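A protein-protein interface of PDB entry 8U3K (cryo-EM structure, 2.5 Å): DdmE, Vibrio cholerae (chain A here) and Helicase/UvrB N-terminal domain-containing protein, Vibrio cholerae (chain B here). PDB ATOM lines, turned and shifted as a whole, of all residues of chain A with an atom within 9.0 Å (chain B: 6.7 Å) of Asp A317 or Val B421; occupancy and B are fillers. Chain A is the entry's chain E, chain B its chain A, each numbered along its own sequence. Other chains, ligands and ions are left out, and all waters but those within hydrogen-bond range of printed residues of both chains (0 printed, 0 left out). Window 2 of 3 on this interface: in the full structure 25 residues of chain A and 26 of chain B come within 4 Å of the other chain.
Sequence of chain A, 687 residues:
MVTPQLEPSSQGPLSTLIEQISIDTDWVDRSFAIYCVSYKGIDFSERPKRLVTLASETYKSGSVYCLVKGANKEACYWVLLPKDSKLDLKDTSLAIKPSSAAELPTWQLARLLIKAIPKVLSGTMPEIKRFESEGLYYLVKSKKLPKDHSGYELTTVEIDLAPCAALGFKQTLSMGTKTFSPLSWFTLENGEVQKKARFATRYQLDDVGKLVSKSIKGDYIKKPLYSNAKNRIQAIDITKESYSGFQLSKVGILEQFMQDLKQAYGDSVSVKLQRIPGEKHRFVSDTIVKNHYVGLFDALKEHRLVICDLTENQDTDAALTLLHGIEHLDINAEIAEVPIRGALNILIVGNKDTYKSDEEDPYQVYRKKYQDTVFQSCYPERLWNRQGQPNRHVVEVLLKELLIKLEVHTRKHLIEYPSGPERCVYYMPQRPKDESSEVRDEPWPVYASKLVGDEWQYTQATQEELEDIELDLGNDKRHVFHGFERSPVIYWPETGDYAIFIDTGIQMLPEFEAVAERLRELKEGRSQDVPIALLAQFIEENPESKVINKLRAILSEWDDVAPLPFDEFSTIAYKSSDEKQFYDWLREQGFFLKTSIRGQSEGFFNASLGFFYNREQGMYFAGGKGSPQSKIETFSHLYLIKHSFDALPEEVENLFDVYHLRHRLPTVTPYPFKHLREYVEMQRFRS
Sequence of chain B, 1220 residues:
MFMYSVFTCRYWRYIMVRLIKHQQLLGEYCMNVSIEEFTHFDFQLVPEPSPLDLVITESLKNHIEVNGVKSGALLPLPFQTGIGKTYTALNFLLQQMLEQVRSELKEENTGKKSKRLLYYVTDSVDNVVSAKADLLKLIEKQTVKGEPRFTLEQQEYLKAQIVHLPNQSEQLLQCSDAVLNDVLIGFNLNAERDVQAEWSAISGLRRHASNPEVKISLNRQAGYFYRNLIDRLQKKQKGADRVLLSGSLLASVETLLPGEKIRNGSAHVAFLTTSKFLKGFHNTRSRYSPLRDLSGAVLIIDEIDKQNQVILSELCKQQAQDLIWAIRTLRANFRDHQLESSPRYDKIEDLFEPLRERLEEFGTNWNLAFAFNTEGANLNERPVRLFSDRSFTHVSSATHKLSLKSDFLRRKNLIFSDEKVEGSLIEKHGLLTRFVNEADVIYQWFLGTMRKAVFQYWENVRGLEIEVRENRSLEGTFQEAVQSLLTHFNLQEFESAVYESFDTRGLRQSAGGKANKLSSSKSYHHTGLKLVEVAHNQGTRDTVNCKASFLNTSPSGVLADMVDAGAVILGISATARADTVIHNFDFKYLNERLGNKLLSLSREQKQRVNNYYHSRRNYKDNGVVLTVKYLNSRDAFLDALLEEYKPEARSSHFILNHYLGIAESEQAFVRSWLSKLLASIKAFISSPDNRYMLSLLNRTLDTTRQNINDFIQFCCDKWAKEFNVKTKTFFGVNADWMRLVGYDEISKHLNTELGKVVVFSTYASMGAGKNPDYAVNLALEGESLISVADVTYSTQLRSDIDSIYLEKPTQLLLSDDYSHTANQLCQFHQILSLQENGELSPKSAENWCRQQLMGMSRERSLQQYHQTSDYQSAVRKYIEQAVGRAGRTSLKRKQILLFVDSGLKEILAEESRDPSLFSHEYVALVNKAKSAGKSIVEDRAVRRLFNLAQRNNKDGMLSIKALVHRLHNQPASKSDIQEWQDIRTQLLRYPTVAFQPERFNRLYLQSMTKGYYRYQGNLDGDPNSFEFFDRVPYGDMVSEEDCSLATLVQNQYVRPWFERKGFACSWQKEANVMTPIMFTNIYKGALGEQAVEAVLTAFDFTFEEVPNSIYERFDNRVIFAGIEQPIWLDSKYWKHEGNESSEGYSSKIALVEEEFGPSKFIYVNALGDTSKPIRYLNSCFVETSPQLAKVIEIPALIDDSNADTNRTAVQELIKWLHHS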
ATOM      1  N   ILE A 307       4.781 -25.983  28.224  1.00  0.00           N
ATOM      2  CA  ILE A 307       3.323 -25.940  28.196  1.00  0.00           C
ATOM      3  C   ILE A 307       2.824 -27.216  27.539  1.00  0.00           C
ATOM      4  O   ILE A 307       3.297 -27.592  26.459  1.00  0.00           O
ATOM      5  CB  ILE A 307       2.805 -24.707  27.442  1.00  0.00           C
ATOM      6  CG1 ILE A 307       3.327 -23.432  28.087  1.00  0.00           C
ATOM      7  CG2 ILE A 307       1.291 -24.703  27.420  1.00  0.00           C
ATOM      8  CD1 ILE A 307       2.787 -23.219  29.467  1.00  0.00           C
ATOM      9  N   ASP A 309      -0.860 -29.777  26.850  1.00  0.00           N
ATOM     10  CA  ASP A 309      -2.314 -29.830  26.773  1.00  0.00           C
ATOM     11  C   ASP A 309      -2.744 -31.289  26.737  1.00  0.00           C
ATOM     12  O   ASP A 309      -2.706 -31.926  25.679  1.00  0.00           O
ATOM     13  CB  ASP A 309      -2.820 -29.078  25.542  1.00  0.00           C
ATOM     14  CG  ASP A 309      -4.323 -28.869  25.550  1.00  0.00           C
ATOM     15  OD1 ASP A 309      -5.020 -29.437  26.415  1.00  0.00           O
ATOM     16  OD2 ASP A 309      -4.813 -28.116  24.685  1.00  0.00           O
ATOM     17  N   THR A 311      -5.840 -32.354  27.930  1.00  0.00           N
ATOM     18  CA  THR A 311      -7.282 -32.522  27.926  1.00  0.00           C
ATOM     19  C   THR A 311      -7.676 -33.563  26.888  1.00  0.00           C
ATOM     20  O   THR A 311      -7.145 -33.583  25.774  1.00  0.00           O
ATOM     21  CB  THR A 311      -7.967 -31.195  27.615  1.00  0.00           C
ATOM     22  OG1 THR A 311      -7.160 -30.447  26.699  1.00  0.00           O
ATOM     23  CG2 THR A 311      -8.165 -30.386  28.882  1.00  0.00           C
ATOM     24  N   ASN A 313      -9.794 -34.996  23.987  1.00  0.00           N
ATOM     25  CA  ASN A 313     -10.379 -34.290  22.848  1.00  0.00           C
ATOM     26  C   ASN A 313      -9.963 -32.816  22.855  1.00  0.00           C
ATOM     27  O   ASN A 313     -10.766 -31.908  23.066  1.00  0.00           O
ATOM     28  CB  ASN A 313     -11.904 -34.442  22.826  1.00  0.00           C
ATOM     29  CG  ASN A 313     -12.506 -34.059  21.489  1.00  0.00           C
ATOM     30  OD1 ASN A 313     -11.788 -33.790  20.526  1.00  0.00           O
ATOM     31  ND2 ASN A 313     -13.831 -34.032  21.424  1.00  0.00           N
ATOM     32  N   GLN A 314      -8.657 -32.623  22.654  1.00  0.00           N
ATOM     33  CA  GLN A 314      -8.081 -31.286  22.573  1.00  0.00           C
ATOM     34  C   GLN A 314      -8.793 -30.458  21.515  1.00  0.00           C
ATOM     35  O   GLN A 314      -8.740 -30.765  20.322  1.00  0.00           O
ATOM     36  CB  GLN A 314      -6.592 -31.378  22.243  1.00  0.00           C
ATOM     37  CG  GLN A 314      -5.852 -32.434  23.033  1.00  0.00           C
ATOM     38  CD  GLN A 314      -4.435 -32.632  22.544  1.00  0.00           C
ATOM     39  OE1 GLN A 314      -3.828 -31.721  21.985  1.00  0.00           O
ATOM     40  NE2 GLN A 314      -3.895 -33.824  22.760  1.00  0.00           N
ATOM     41  N   ASP A 315      -9.464 -29.399  21.961  1.00  0.00           N
ATOM     42  CA  ASP A 315     -10.390 -28.691  21.090  1.00  0.00           C
ATOM     43  C   ASP A 315     -10.110 -27.196  21.000  1.00  0.00           C
ATOM     44  O   ASP A 315     -10.249 -26.600  19.928  1.00  0.00           O
ATOM     45  CB  ASP A 315     -11.822 -28.919  21.579  1.00  0.00           C
ATOM     46  CG  ASP A 315     -12.857 -28.417  20.600  1.00  0.00           C
ATOM     47  OD1 ASP A 315     -12.558 -28.359  19.389  1.00  0.00           O
ATOM     48  OD2 ASP A 315     -13.973 -28.075  21.043  1.00  0.00           O
ATOM     49  N   THR A 316      -9.713 -26.579  22.111  1.00  0.00           N
ATOM     50  CA  THR A 316      -9.678 -25.125  22.183  1.00  0.00           C
ATOM     51  C   THR A 316      -8.337 -24.522  21.791  1.00  0.00           C
ATOM     52  O   THR A 316      -8.287 -23.317  21.519  1.00  0.00           O
ATOM     53  CB  THR A 316     -10.040 -24.664  23.595  1.00  0.00           C
ATOM     54  OG1 THR A 316      -9.118 -25.233  24.533  1.00  0.00           O
ATOM     55  CG2 THR A 316     -11.448 -25.105  23.950  1.00  0.00           C
ATOM     56  N   ASP A 317      -7.269 -25.321  21.750  1.00  0.00           N
ATOM     57  CA  ASP A 317      -5.908 -24.829  21.516  1.00  0.00           C
ATOM     58  C   ASP A 317      -5.550 -23.719  22.497  1.00  0.00           C
ATOM     59  O   ASP A 317      -4.923 -22.717  22.143  1.00  0.00           O
ATOM     60  CB  ASP A 317      -5.717 -24.367  20.070  1.00  0.00           C
ATOM     61  CG  ASP A 317      -5.795 -25.509  19.083  1.00  0.00           C
ATOM     62  OD1 ASP A 317      -5.649 -26.674  19.510  1.00  0.00           O
ATOM     63  OD2 ASP A 317      -5.991 -25.242  17.879  1.00  0.00           O
ATOM     64  N   ALA A 318      -5.965 -23.903  23.752  1.00  0.00           N
ATOM     65  CA  ALA A 318      -5.660 -22.928  24.790  1.00  0.00           C
ATOM     66  C   ALA A 318      -4.172 -22.887  25.095  1.00  0.00           C
ATOM     67  O   ALA A 318      -3.685 -21.904  25.662  1.00  0.00           O
ATOM     68  CB  ALA A 318      -6.455 -23.251  26.051  1.00  0.00           C
ATOM     69  N   ALA A 319      -3.440 -23.943  24.735  1.00  0.00           N
ATOM     70  CA  ALA A 319      -1.998 -23.963  24.951  1.00  0.00           C
ATOM     71  C   ALA A 319      -1.317 -22.858  24.158  1.00  0.00           C
ATOM     72  O   ALA A 319      -0.378 -22.214  24.642  1.00  0.00           O
ATOM     73  CB  ALA A 319      -1.435 -25.330  24.575  1.00  0.00           C
ATOM     74  N   LEU A 320      -1.790 -22.615  22.935  1.00  0.00           N
ATOM     75  CA  LEU A 320      -1.272 -21.500  22.152  1.00  0.00           C
ATOM     76  C   LEU A 320      -1.541 -20.168  22.839  1.00  0.00           C
ATOM     77  O   LEU A 320      -0.683 -19.277  22.822  1.00  0.00           O
ATOM     78  CB  LEU A 320      -1.890 -21.511  20.756  1.00  0.00           C
ATOM     79  CG  LEU A 320      -1.277 -20.540  19.748  1.00  0.00           C
ATOM     80  CD1 LEU A 320       0.195 -20.857  19.532  1.00  0.00           C
ATOM     81  CD2 LEU A 320      -2.038 -20.581  18.438  1.00  0.00           C
ATOM     82  N   THR A 321      -2.717 -20.022  23.451  1.00  0.00           N
ATOM     83  CA  THR A 321      -3.028 -18.804  24.190  1.00  0.00           C
ATOM     84  C   THR A 321      -2.103 -18.629  25.384  1.00  0.00           C
ATOM     85  O   THR A 321      -1.635 -17.517  25.657  1.00  0.00           O
ATOM     86  CB  THR A 321      -4.481 -18.835  24.645  1.00  0.00           C
ATOM     87  OG1 THR A 321      -5.309 -19.209  23.540  1.00  0.00           O
ATOM     88  CG2 THR A 321      -4.900 -17.474  25.144  1.00  0.00           C
ATOM     89  N   LEU A 322      -1.836 -19.715  26.110  1.00  0.00           N
ATOM     90  CA  LEU A 322      -0.901 -19.650  27.226  1.00  0.00           C
ATOM     91  C   LEU A 322       0.482 -19.239  26.751  1.00  0.00           C
ATOM     92  O   LEU A 322       1.150 -18.421  27.390  1.00  0.00           O
ATOM     93  CB  LEU A 322      -0.834 -20.996  27.944  1.00  0.00           C
ATOM     94  CG  LEU A 322      -1.247 -21.007  29.413  1.00  0.00           C
ATOM     95  CD1 LEU A 322      -2.747 -20.876  29.561  1.00  0.00           C
ATOM     96  CD2 LEU A 322      -0.749 -22.269  30.081  1.00  0.00           C
ATOM     97  N   LEU A 323       0.926 -19.798  25.625  1.00  0.00           N
ATOM     98  CA  LEU A 323       2.243 -19.455  25.100  1.00  0.00           C
ATOM     99  C   LEU A 323       2.305 -17.984  24.707  1.00  0.00           C
ATOM    100  O   LEU A 323       3.291 -17.293  24.993  1.00  0.00           O
ATOM    101  CB  LEU A 323       2.576 -20.359  23.912  1.00  0.00           C
ATOM    102  CG  LEU A 323       4.040 -20.505  23.492  1.00  0.00           C
ATOM    103  CD1 LEU A 323       4.518 -19.375  22.587  1.00  0.00           C
ATOM    104  CD2 LEU A 323       4.911 -20.593  24.727  1.00  0.00           C
ATOM    105  N   HIS A 324       1.250 -17.488  24.057  1.00  0.00           N
ATOM    106  CA  HIS A 324       1.211 -16.091  23.639  1.00  0.00           C
ATOM    107  C   HIS A 324       1.228 -15.161  24.847  1.00  0.00           C
ATOM    108  O   HIS A 324       1.946 -14.151  24.864  1.00  0.00           O
ATOM    109  CB  HIS A 324      -0.032 -15.847  22.783  1.00  0.00           C
ATOM    110  CG  HIS A 324      -0.109 -14.474  22.194  1.00  0.00           C
ATOM    111  ND1 HIS A 324       1.010 -13.740  21.864  1.00  0.00           N
ATOM    112  CD2 HIS A 324      -1.173 -13.700  21.874  1.00  0.00           C
ATOM    113  CE1 HIS A 324       0.638 -12.577  21.362  1.00  0.00           C
ATOM    114  NE2 HIS A 324      -0.681 -12.526  21.361  1.00  0.00           N
ATOM    115  N   ILE A 335       5.774 -25.253  23.625  1.00  0.00           N
ATOM    116  CA  ILE A 335       4.686 -26.210  23.729  1.00  0.00           C
ATOM    117  C   ILE A 335       5.239 -27.609  23.489  1.00  0.00           C
ATOM    118  O   ILE A 335       6.160 -27.808  22.688  1.00  0.00           O
ATOM    119  CB  ILE A 335       3.585 -25.860  22.713  1.00  0.00           C
ATOM    120  CG1 ILE A 335       3.150 -24.406  22.898  1.00  0.00           C
ATOM    121  CG2 ILE A 335       2.396 -26.806  22.838  1.00  0.00           C
ATOM    122  CD1 ILE A 335       1.967 -24.217  23.793  1.00  0.00           C
ATOM    123  N   GLU A 337       4.036 -32.067  23.518  1.00  0.00           N
ATOM    124  CA  GLU A 337       2.969 -33.053  23.590  1.00  0.00           C
ATOM    125  C   GLU A 337       2.916 -33.734  24.948  1.00  0.00           C
ATOM    126  O   GLU A 337       1.829 -34.078  25.422  1.00  0.00           O
ATOM    127  CB  GLU A 337       3.147 -34.094  22.486  1.00  0.00           C
ATOM    128  CG  GLU A 337       3.308 -33.498  21.096  1.00  0.00           C
ATOM    129  CD  GLU A 337       2.142 -32.616  20.695  1.00  0.00           C
ATOM    130  OE1 GLU A 337       0.986 -32.982  20.993  1.00  0.00           O
ATOM    131  OE2 GLU A 337       2.382 -31.554  20.083  1.00  0.00           O
ATOM    132  N   ILE A 348      -2.438 -28.406  31.024  1.00  0.00           N
ATOM    133  CA  ILE A 348      -3.836 -28.039  30.856  1.00  0.00           C
ATOM    134  C   ILE A 348      -4.655 -29.320  30.834  1.00  0.00           C
ATOM    135  O   ILE A 348      -4.719 -30.012  29.812  1.00  0.00           O
ATOM    136  CB  ILE A 348      -4.050 -27.221  29.581  1.00  0.00           C
ATOM    137  CG1 ILE A 348      -3.035 -26.088  29.511  1.00  0.00           C
ATOM    138  CG2 ILE A 348      -5.448 -26.666  29.562  1.00  0.00           C
ATOM    139  CD1 ILE A 348      -3.229 -25.184  28.333  1.00  0.00           C
ATOM    140  N   PRO A 380      -8.818 -25.472  30.751  1.00  0.00           N
ATOM    141  CA  PRO A 380      -8.756 -24.609  29.574  1.00  0.00           C
ATOM    142  C   PRO A 380      -9.869 -23.569  29.456  1.00  0.00           C
ATOM    143  O   PRO A 380      -9.766 -22.700  28.582  1.00  0.00           O
ATOM    144  CB  PRO A 380      -8.756 -25.628  28.433  1.00  0.00           C
ATOM    145  CG  PRO A 380      -9.588 -26.820  29.014  1.00  0.00           C
ATOM    146  CD  PRO A 380      -9.874 -26.463  30.472  1.00  0.00           C
ATOM    147  N   LEU A 383      -8.858 -19.343  30.940  1.00  0.00           N
ATOM    148  CA  LEU A 383      -7.973 -18.329  30.378  1.00  0.00           C
ATOM    149  C   LEU A 383      -8.723 -17.401  29.431  1.00  0.00           C
ATOM    150  O   LEU A 383      -8.085 -16.657  28.678  1.00  0.00           O
ATOM    151  CB  LEU A 383      -6.783 -18.983  29.696  1.00  0.00           C
ATOM    152  CG  LEU A 383      -7.117 -20.206  28.865  1.00  0.00           C
ATOM    153  CD1 LEU A 383      -6.835 -19.904  27.408  1.00  0.00           C
ATOM    154  CD2 LEU A 383      -6.327 -21.398  29.357  1.00  0.00           C
ATOM    155  N   TRP A 384     -10.052 -17.421  29.457  1.00  0.00           N
ATOM    156  CA  TRP A 384     -10.892 -16.557  28.645  1.00  0.00           C
ATOM    157  C   TRP A 384     -11.658 -15.609  29.547  1.00  0.00           C
ATOM    158  O   TRP A 384     -12.141 -16.003  30.611  1.00  0.00           O
ATOM    159  CB  TRP A 384     -11.902 -17.361  27.811  1.00  0.00           C
ATOM    160  CG  TRP A 384     -11.335 -18.499  27.021  1.00  0.00           C
ATOM    161  CD1 TRP A 384     -11.824 -19.769  26.967  1.00  0.00           C
ATOM    162  CD2 TRP A 384     -10.245 -18.453  26.094  1.00  0.00           C
ATOM    163  NE1 TRP A 384     -11.070 -20.533  26.115  1.00  0.00           N
ATOM    164  CE2 TRP A 384     -10.097 -19.747  25.563  1.00  0.00           C
ATOM    165  CE3 TRP A 384      -9.365 -17.451  25.681  1.00  0.00           C
ATOM    166  CZ2 TRP A 384      -9.112 -20.062  24.644  1.00  0.00           C
ATOM    167  CZ3 TRP A 384      -8.390 -17.769  24.772  1.00  0.00           C
ATOM    168  CH2 TRP A 384      -8.270 -19.062  24.260  1.00  0.00           C
ATOM    169  N   ALA B 398     -11.892 -26.221  11.368  1.00  0.00           N
ATOM    170  CA  ALA B 398     -10.985 -27.180  11.969  1.00  0.00           C
ATOM    171  C   ALA B 398      -9.703 -26.490  12.397  1.00  0.00           C
ATOM    172  O   ALA B 398      -9.119 -25.705  11.647  1.00  0.00           O
ATOM    173  CB  ALA B 398     -10.669 -28.296  10.982  1.00  0.00           C
ATOM    174  N   THR B 399      -9.265 -26.786  13.618  1.00  0.00           N
ATOM    175  CA  THR B 399      -7.937 -26.357  14.032  1.00  0.00           C
ATOM    176  C   THR B 399      -6.859 -27.053  13.223  1.00  0.00           C
ATOM    177  O   THR B 399      -5.749 -26.535  13.083  1.00  0.00           O
ATOM    178  CB  THR B 399      -7.721 -26.644  15.515  1.00  0.00           C
ATOM    179  OG1 THR B 399      -7.358 -28.017  15.684  1.00  0.00           O
ATOM    180  CG2 THR B 399      -8.983 -26.362  16.299  1.00  0.00           C
ATOM    181  N   HIS B 400      -7.180 -28.207  12.660  1.00  0.00           N
ATOM    182  CA  HIS B 400      -6.179 -29.090  12.107  1.00  0.00           C
ATOM    183  C   HIS B 400      -5.986 -28.844  10.616  1.00  0.00           C
ATOM    184  O   HIS B 400      -6.672 -28.035   9.991  1.00  0.00           O
ATOM    185  CB  HIS B 400      -6.591 -30.537  12.342  1.00  0.00           C
ATOM    186  CG  HIS B 400      -7.053 -30.815  13.738  1.00  0.00           C
ATOM    187  ND1 HIS B 400      -8.312 -30.481  14.187  1.00  0.00           N
ATOM    188  CD2 HIS B 400      -6.419 -31.389  14.788  1.00  0.00           C
ATOM    189  CE1 HIS B 400      -8.438 -30.844  15.451  1.00  0.00           C
ATOM    190  NE2 HIS B 400      -7.302 -31.395  15.840  1.00  0.00           N
ATOM    191  N   LYS B 401      -5.022 -29.561  10.050  1.00  0.00           N
ATOM    192  CA  LYS B 401      -4.836 -29.605   8.604  1.00  0.00           C
ATOM    193  C   LYS B 401      -5.528 -30.860   8.077  1.00  0.00           C
ATOM    194  O   LYS B 401      -4.953 -31.944   7.968  1.00  0.00           O
ATOM    195  CB  LYS B 401      -3.357 -29.588   8.251  1.00  0.00           C
ATOM    196  CG  LYS B 401      -3.076 -29.331   6.785  1.00  0.00           C
ATOM    197  CD  LYS B 401      -1.591 -29.467   6.479  1.00  0.00           C
ATOM    198  CE  LYS B 401      -1.120 -30.898   6.679  1.00  0.00           C
ATOM    199  NZ  LYS B 401       0.267 -31.109   6.181  1.00  0.00           N
ATOM    200  N   ASP B 418      -4.339 -34.561  10.688  1.00  0.00           N
ATOM    201  CA  ASP B 418      -3.046 -34.229  11.269  1.00  0.00           C
ATOM    202  C   ASP B 418      -3.317 -33.302  12.445  1.00  0.00           C
ATOM    203  O   ASP B 418      -4.346 -32.627  12.466  1.00  0.00           O
ATOM    204  CB  ASP B 418      -2.126 -33.580  10.236  1.00  0.00           C
ATOM    205  CG  ASP B 418      -1.447 -34.597   9.349  1.00  0.00           C
ATOM    206  OD1 ASP B 418      -1.634 -35.808   9.587  1.00  0.00           O
ATOM    207  OD2 ASP B 418      -0.736 -34.191   8.408  1.00  0.00           O
ATOM    208  N   GLU B 419      -2.426 -33.255  13.435  1.00  0.00           N
ATOM    209  CA  GLU B 419      -2.781 -32.595  14.689  1.00  0.00           C
ATOM    210  C   GLU B 419      -2.461 -31.103  14.669  1.00  0.00           C
ATOM    211  O   GLU B 419      -2.137 -30.519  15.709  1.00  0.00           O
ATOM    212  CB  GLU B 419      -2.087 -33.282  15.864  1.00  0.00           C
ATOM    213  CG  GLU B 419      -2.728 -34.610  16.235  1.00  0.00           C
ATOM    214  CD  GLU B 419      -4.052 -34.431  16.957  1.00  0.00           C
ATOM    215  OE1 GLU B 419      -4.087 -33.704  17.971  1.00  0.00           O
ATOM    216  OE2 GLU B 419      -5.060 -35.014  16.502  1.00  0.00           O
ATOM    217  N   LYS B 420      -2.533 -30.476  13.492  1.00  0.00           N
ATOM    218  CA  LYS B 420      -2.220 -29.060  13.313  1.00  0.00           C
ATOM    219  C   LYS B 420      -3.059 -28.154  14.212  1.00  0.00           C
ATOM    220  O   LYS B 420      -4.165 -28.519  14.621  1.00  0.00           O
ATOM    221  CB  LYS B 420      -2.422 -28.660  11.850  1.00  0.00           C
ATOM    222  CG  LYS B 420      -1.483 -27.566  11.368  1.00  0.00           C
ATOM    223  CD  LYS B 420      -2.228 -26.274  11.071  1.00  0.00           C
ATOM    224  CE  LYS B 420      -3.223 -26.427   9.936  1.00  0.00           C
ATOM    225  NZ  LYS B 420      -3.973 -25.163   9.702  1.00  0.00           N
ATOM    226  N   VAL B 421      -2.538 -26.965  14.508  1.00  0.00           N
ATOM    227  CA  VAL B 421      -3.152 -26.043  15.460  1.00  0.00           C
ATOM    228  C   VAL B 421      -3.852 -24.945  14.668  1.00  0.00           C
ATOM    229  O   VAL B 421      -3.438 -24.604  13.557  1.00  0.00           O
ATOM    230  CB  VAL B 421      -2.088 -25.483  16.439  1.00  0.00           C
ATOM    231  CG1 VAL B 421      -0.969 -24.781  15.678  1.00  0.00           C
ATOM    232  CG2 VAL B 421      -2.705 -24.574  17.502  1.00  0.00           C
ATOM    233  N   GLU B 422      -4.941 -24.410  15.238  1.00  0.00           N
ATOM    234  CA  GLU B 422      -5.758 -23.428  14.526  1.00  0.00           C
ATOM    235  C   GLU B 422      -4.996 -22.137  14.262  1.00  0.00           C
ATOM    236  O   GLU B 422      -5.311 -21.416  13.308  1.00  0.00           O
ATOM    237  CB  GLU B 422      -7.031 -23.128  15.323  1.00  0.00           C
ATOM    238  CG  GLU B 422      -8.224 -22.678  14.480  1.00  0.00           C
ATOM    239  CD  GLU B 422      -8.423 -21.179  14.461  1.00  0.00           C
ATOM    240  OE1 GLU B 422      -7.823 -20.482  15.305  1.00  0.00           O
ATOM    241  OE2 GLU B 422      -9.201 -20.701  13.610  1.00  0.00           O
ATOM    242  N   GLY B 423      -4.001 -21.824  15.097  1.00  0.00           N
ATOM    243  CA  GLY B 423      -3.254 -20.587  14.948  1.00  0.00           C
ATOM    244  C   GLY B 423      -2.420 -20.509  13.687  1.00  0.00           C
ATOM    245  O   GLY B 423      -2.332 -19.433  13.085  1.00  0.00           O
ATOM    246  N   SER B 424      -1.810 -21.616  13.273  1.00  0.00           N
ATOM    247  CA  SER B 424      -0.984 -21.635  12.065  1.00  0.00           C
ATOM    248  C   SER B 424      -1.822 -21.930  10.823  1.00  0.00           C
ATOM    249  O   SER B 424      -1.619 -22.923  10.126  1.00  0.00           O
ATOM    250  CB  SER B 424       0.144 -22.648  12.221  1.00  0.00           C
ATOM    251  OG  SER B 424      -0.359 -23.965  12.350  1.00  0.00           O
ATOM    252  N   LEU B 425      -2.779 -21.043  10.539  1.00  0.00           N
ATOM    253  CA  LEU B 425      -3.630 -21.192   9.365  1.00  0.00           C
ATOM    254  C   LEU B 425      -2.892 -20.879   8.068  1.00  0.00           C
ATOM    255  O   LEU B 425      -3.432 -21.139   6.987  1.00  0.00           O
ATOM    256  CB  LEU B 425      -4.863 -20.293   9.508  1.00  0.00           C
ATOM    257  CG  LEU B 425      -6.124 -20.645   8.711  1.00  0.00           C
ATOM    258  CD1 LEU B 425      -6.507 -22.103   8.910  1.00  0.00           C
ATOM    259  CD2 LEU B 425      -7.268 -19.733   9.106  1.00  0.00           C
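Of the 12 printed residues of chain B, 4 touch a printed residue of chain A. Hydrophobic or aromatic side chains of chain B within 4 Å of the printed part of chain A: Val B421. Of the 21 printed residues of chain A, 3 touch a printed residue of chain B. Printed residues of chain A that touch a printed residue of chain B: Asp A315, Asp A317 and Leu A320. Hydrophobic or aromatic side chains of chain A within 4 Å of the printed part of chain B: Leu A320. Among the printed residues, 5 pairs touch across the chains.
OG1 of Thr B399 lies close to ND1 of His B400. The side-chain hydroxyl of Thr B399 lies close to the backbone carbonyl oxygen of Lys B420 (3.4 Å). The backbone NH (N) of Glu B422 sits at hydrogen-bond distance from the backbone carbonyl oxygen (O) of Thr B399, 3.1 Å away. O of Val B421 lies within hydrogen-bond range of OG of Ser B424 (3.4 Å).
Thr B399 touches Asp A315. OD2 of Asp A317 touches CB of Thr B399 (3.2 Å). Asp A317 touches Val B421. Leu A320 touches Gly B423.
Of chain B, only Thr B399 (3.2 Å), Val B421 (3.4 Å) and Glu B422 (3.0 Å) come within 4 Å of Asp A317. Val B421 touches just one residue of chain A: Asp A317 (3.4 Å). No residue of chain A comes within 4 Å of Lys B420. No residue of chain A comes within 4 Å of Ser B424. Of the printed residues of chain A, Glu B422 touches Asp A317. Of the printed residues of chain A, Gly B423 touches Leu A320. Printed residues of chain B within 4 Å of Asp A315: Thr B399 (3.9 Å). Printed residues of chain B within 4 Å of Leu A320: Gly B423 (3.7 Å). The nearest printed residue of chain A that does not touch Gly B423 is Asp A317 (4.8 Å).
The side-chain carboxylate (OD2) of Asp A317 lies within hydrogen-bond range of the backbone NH (N) of Glu B422.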
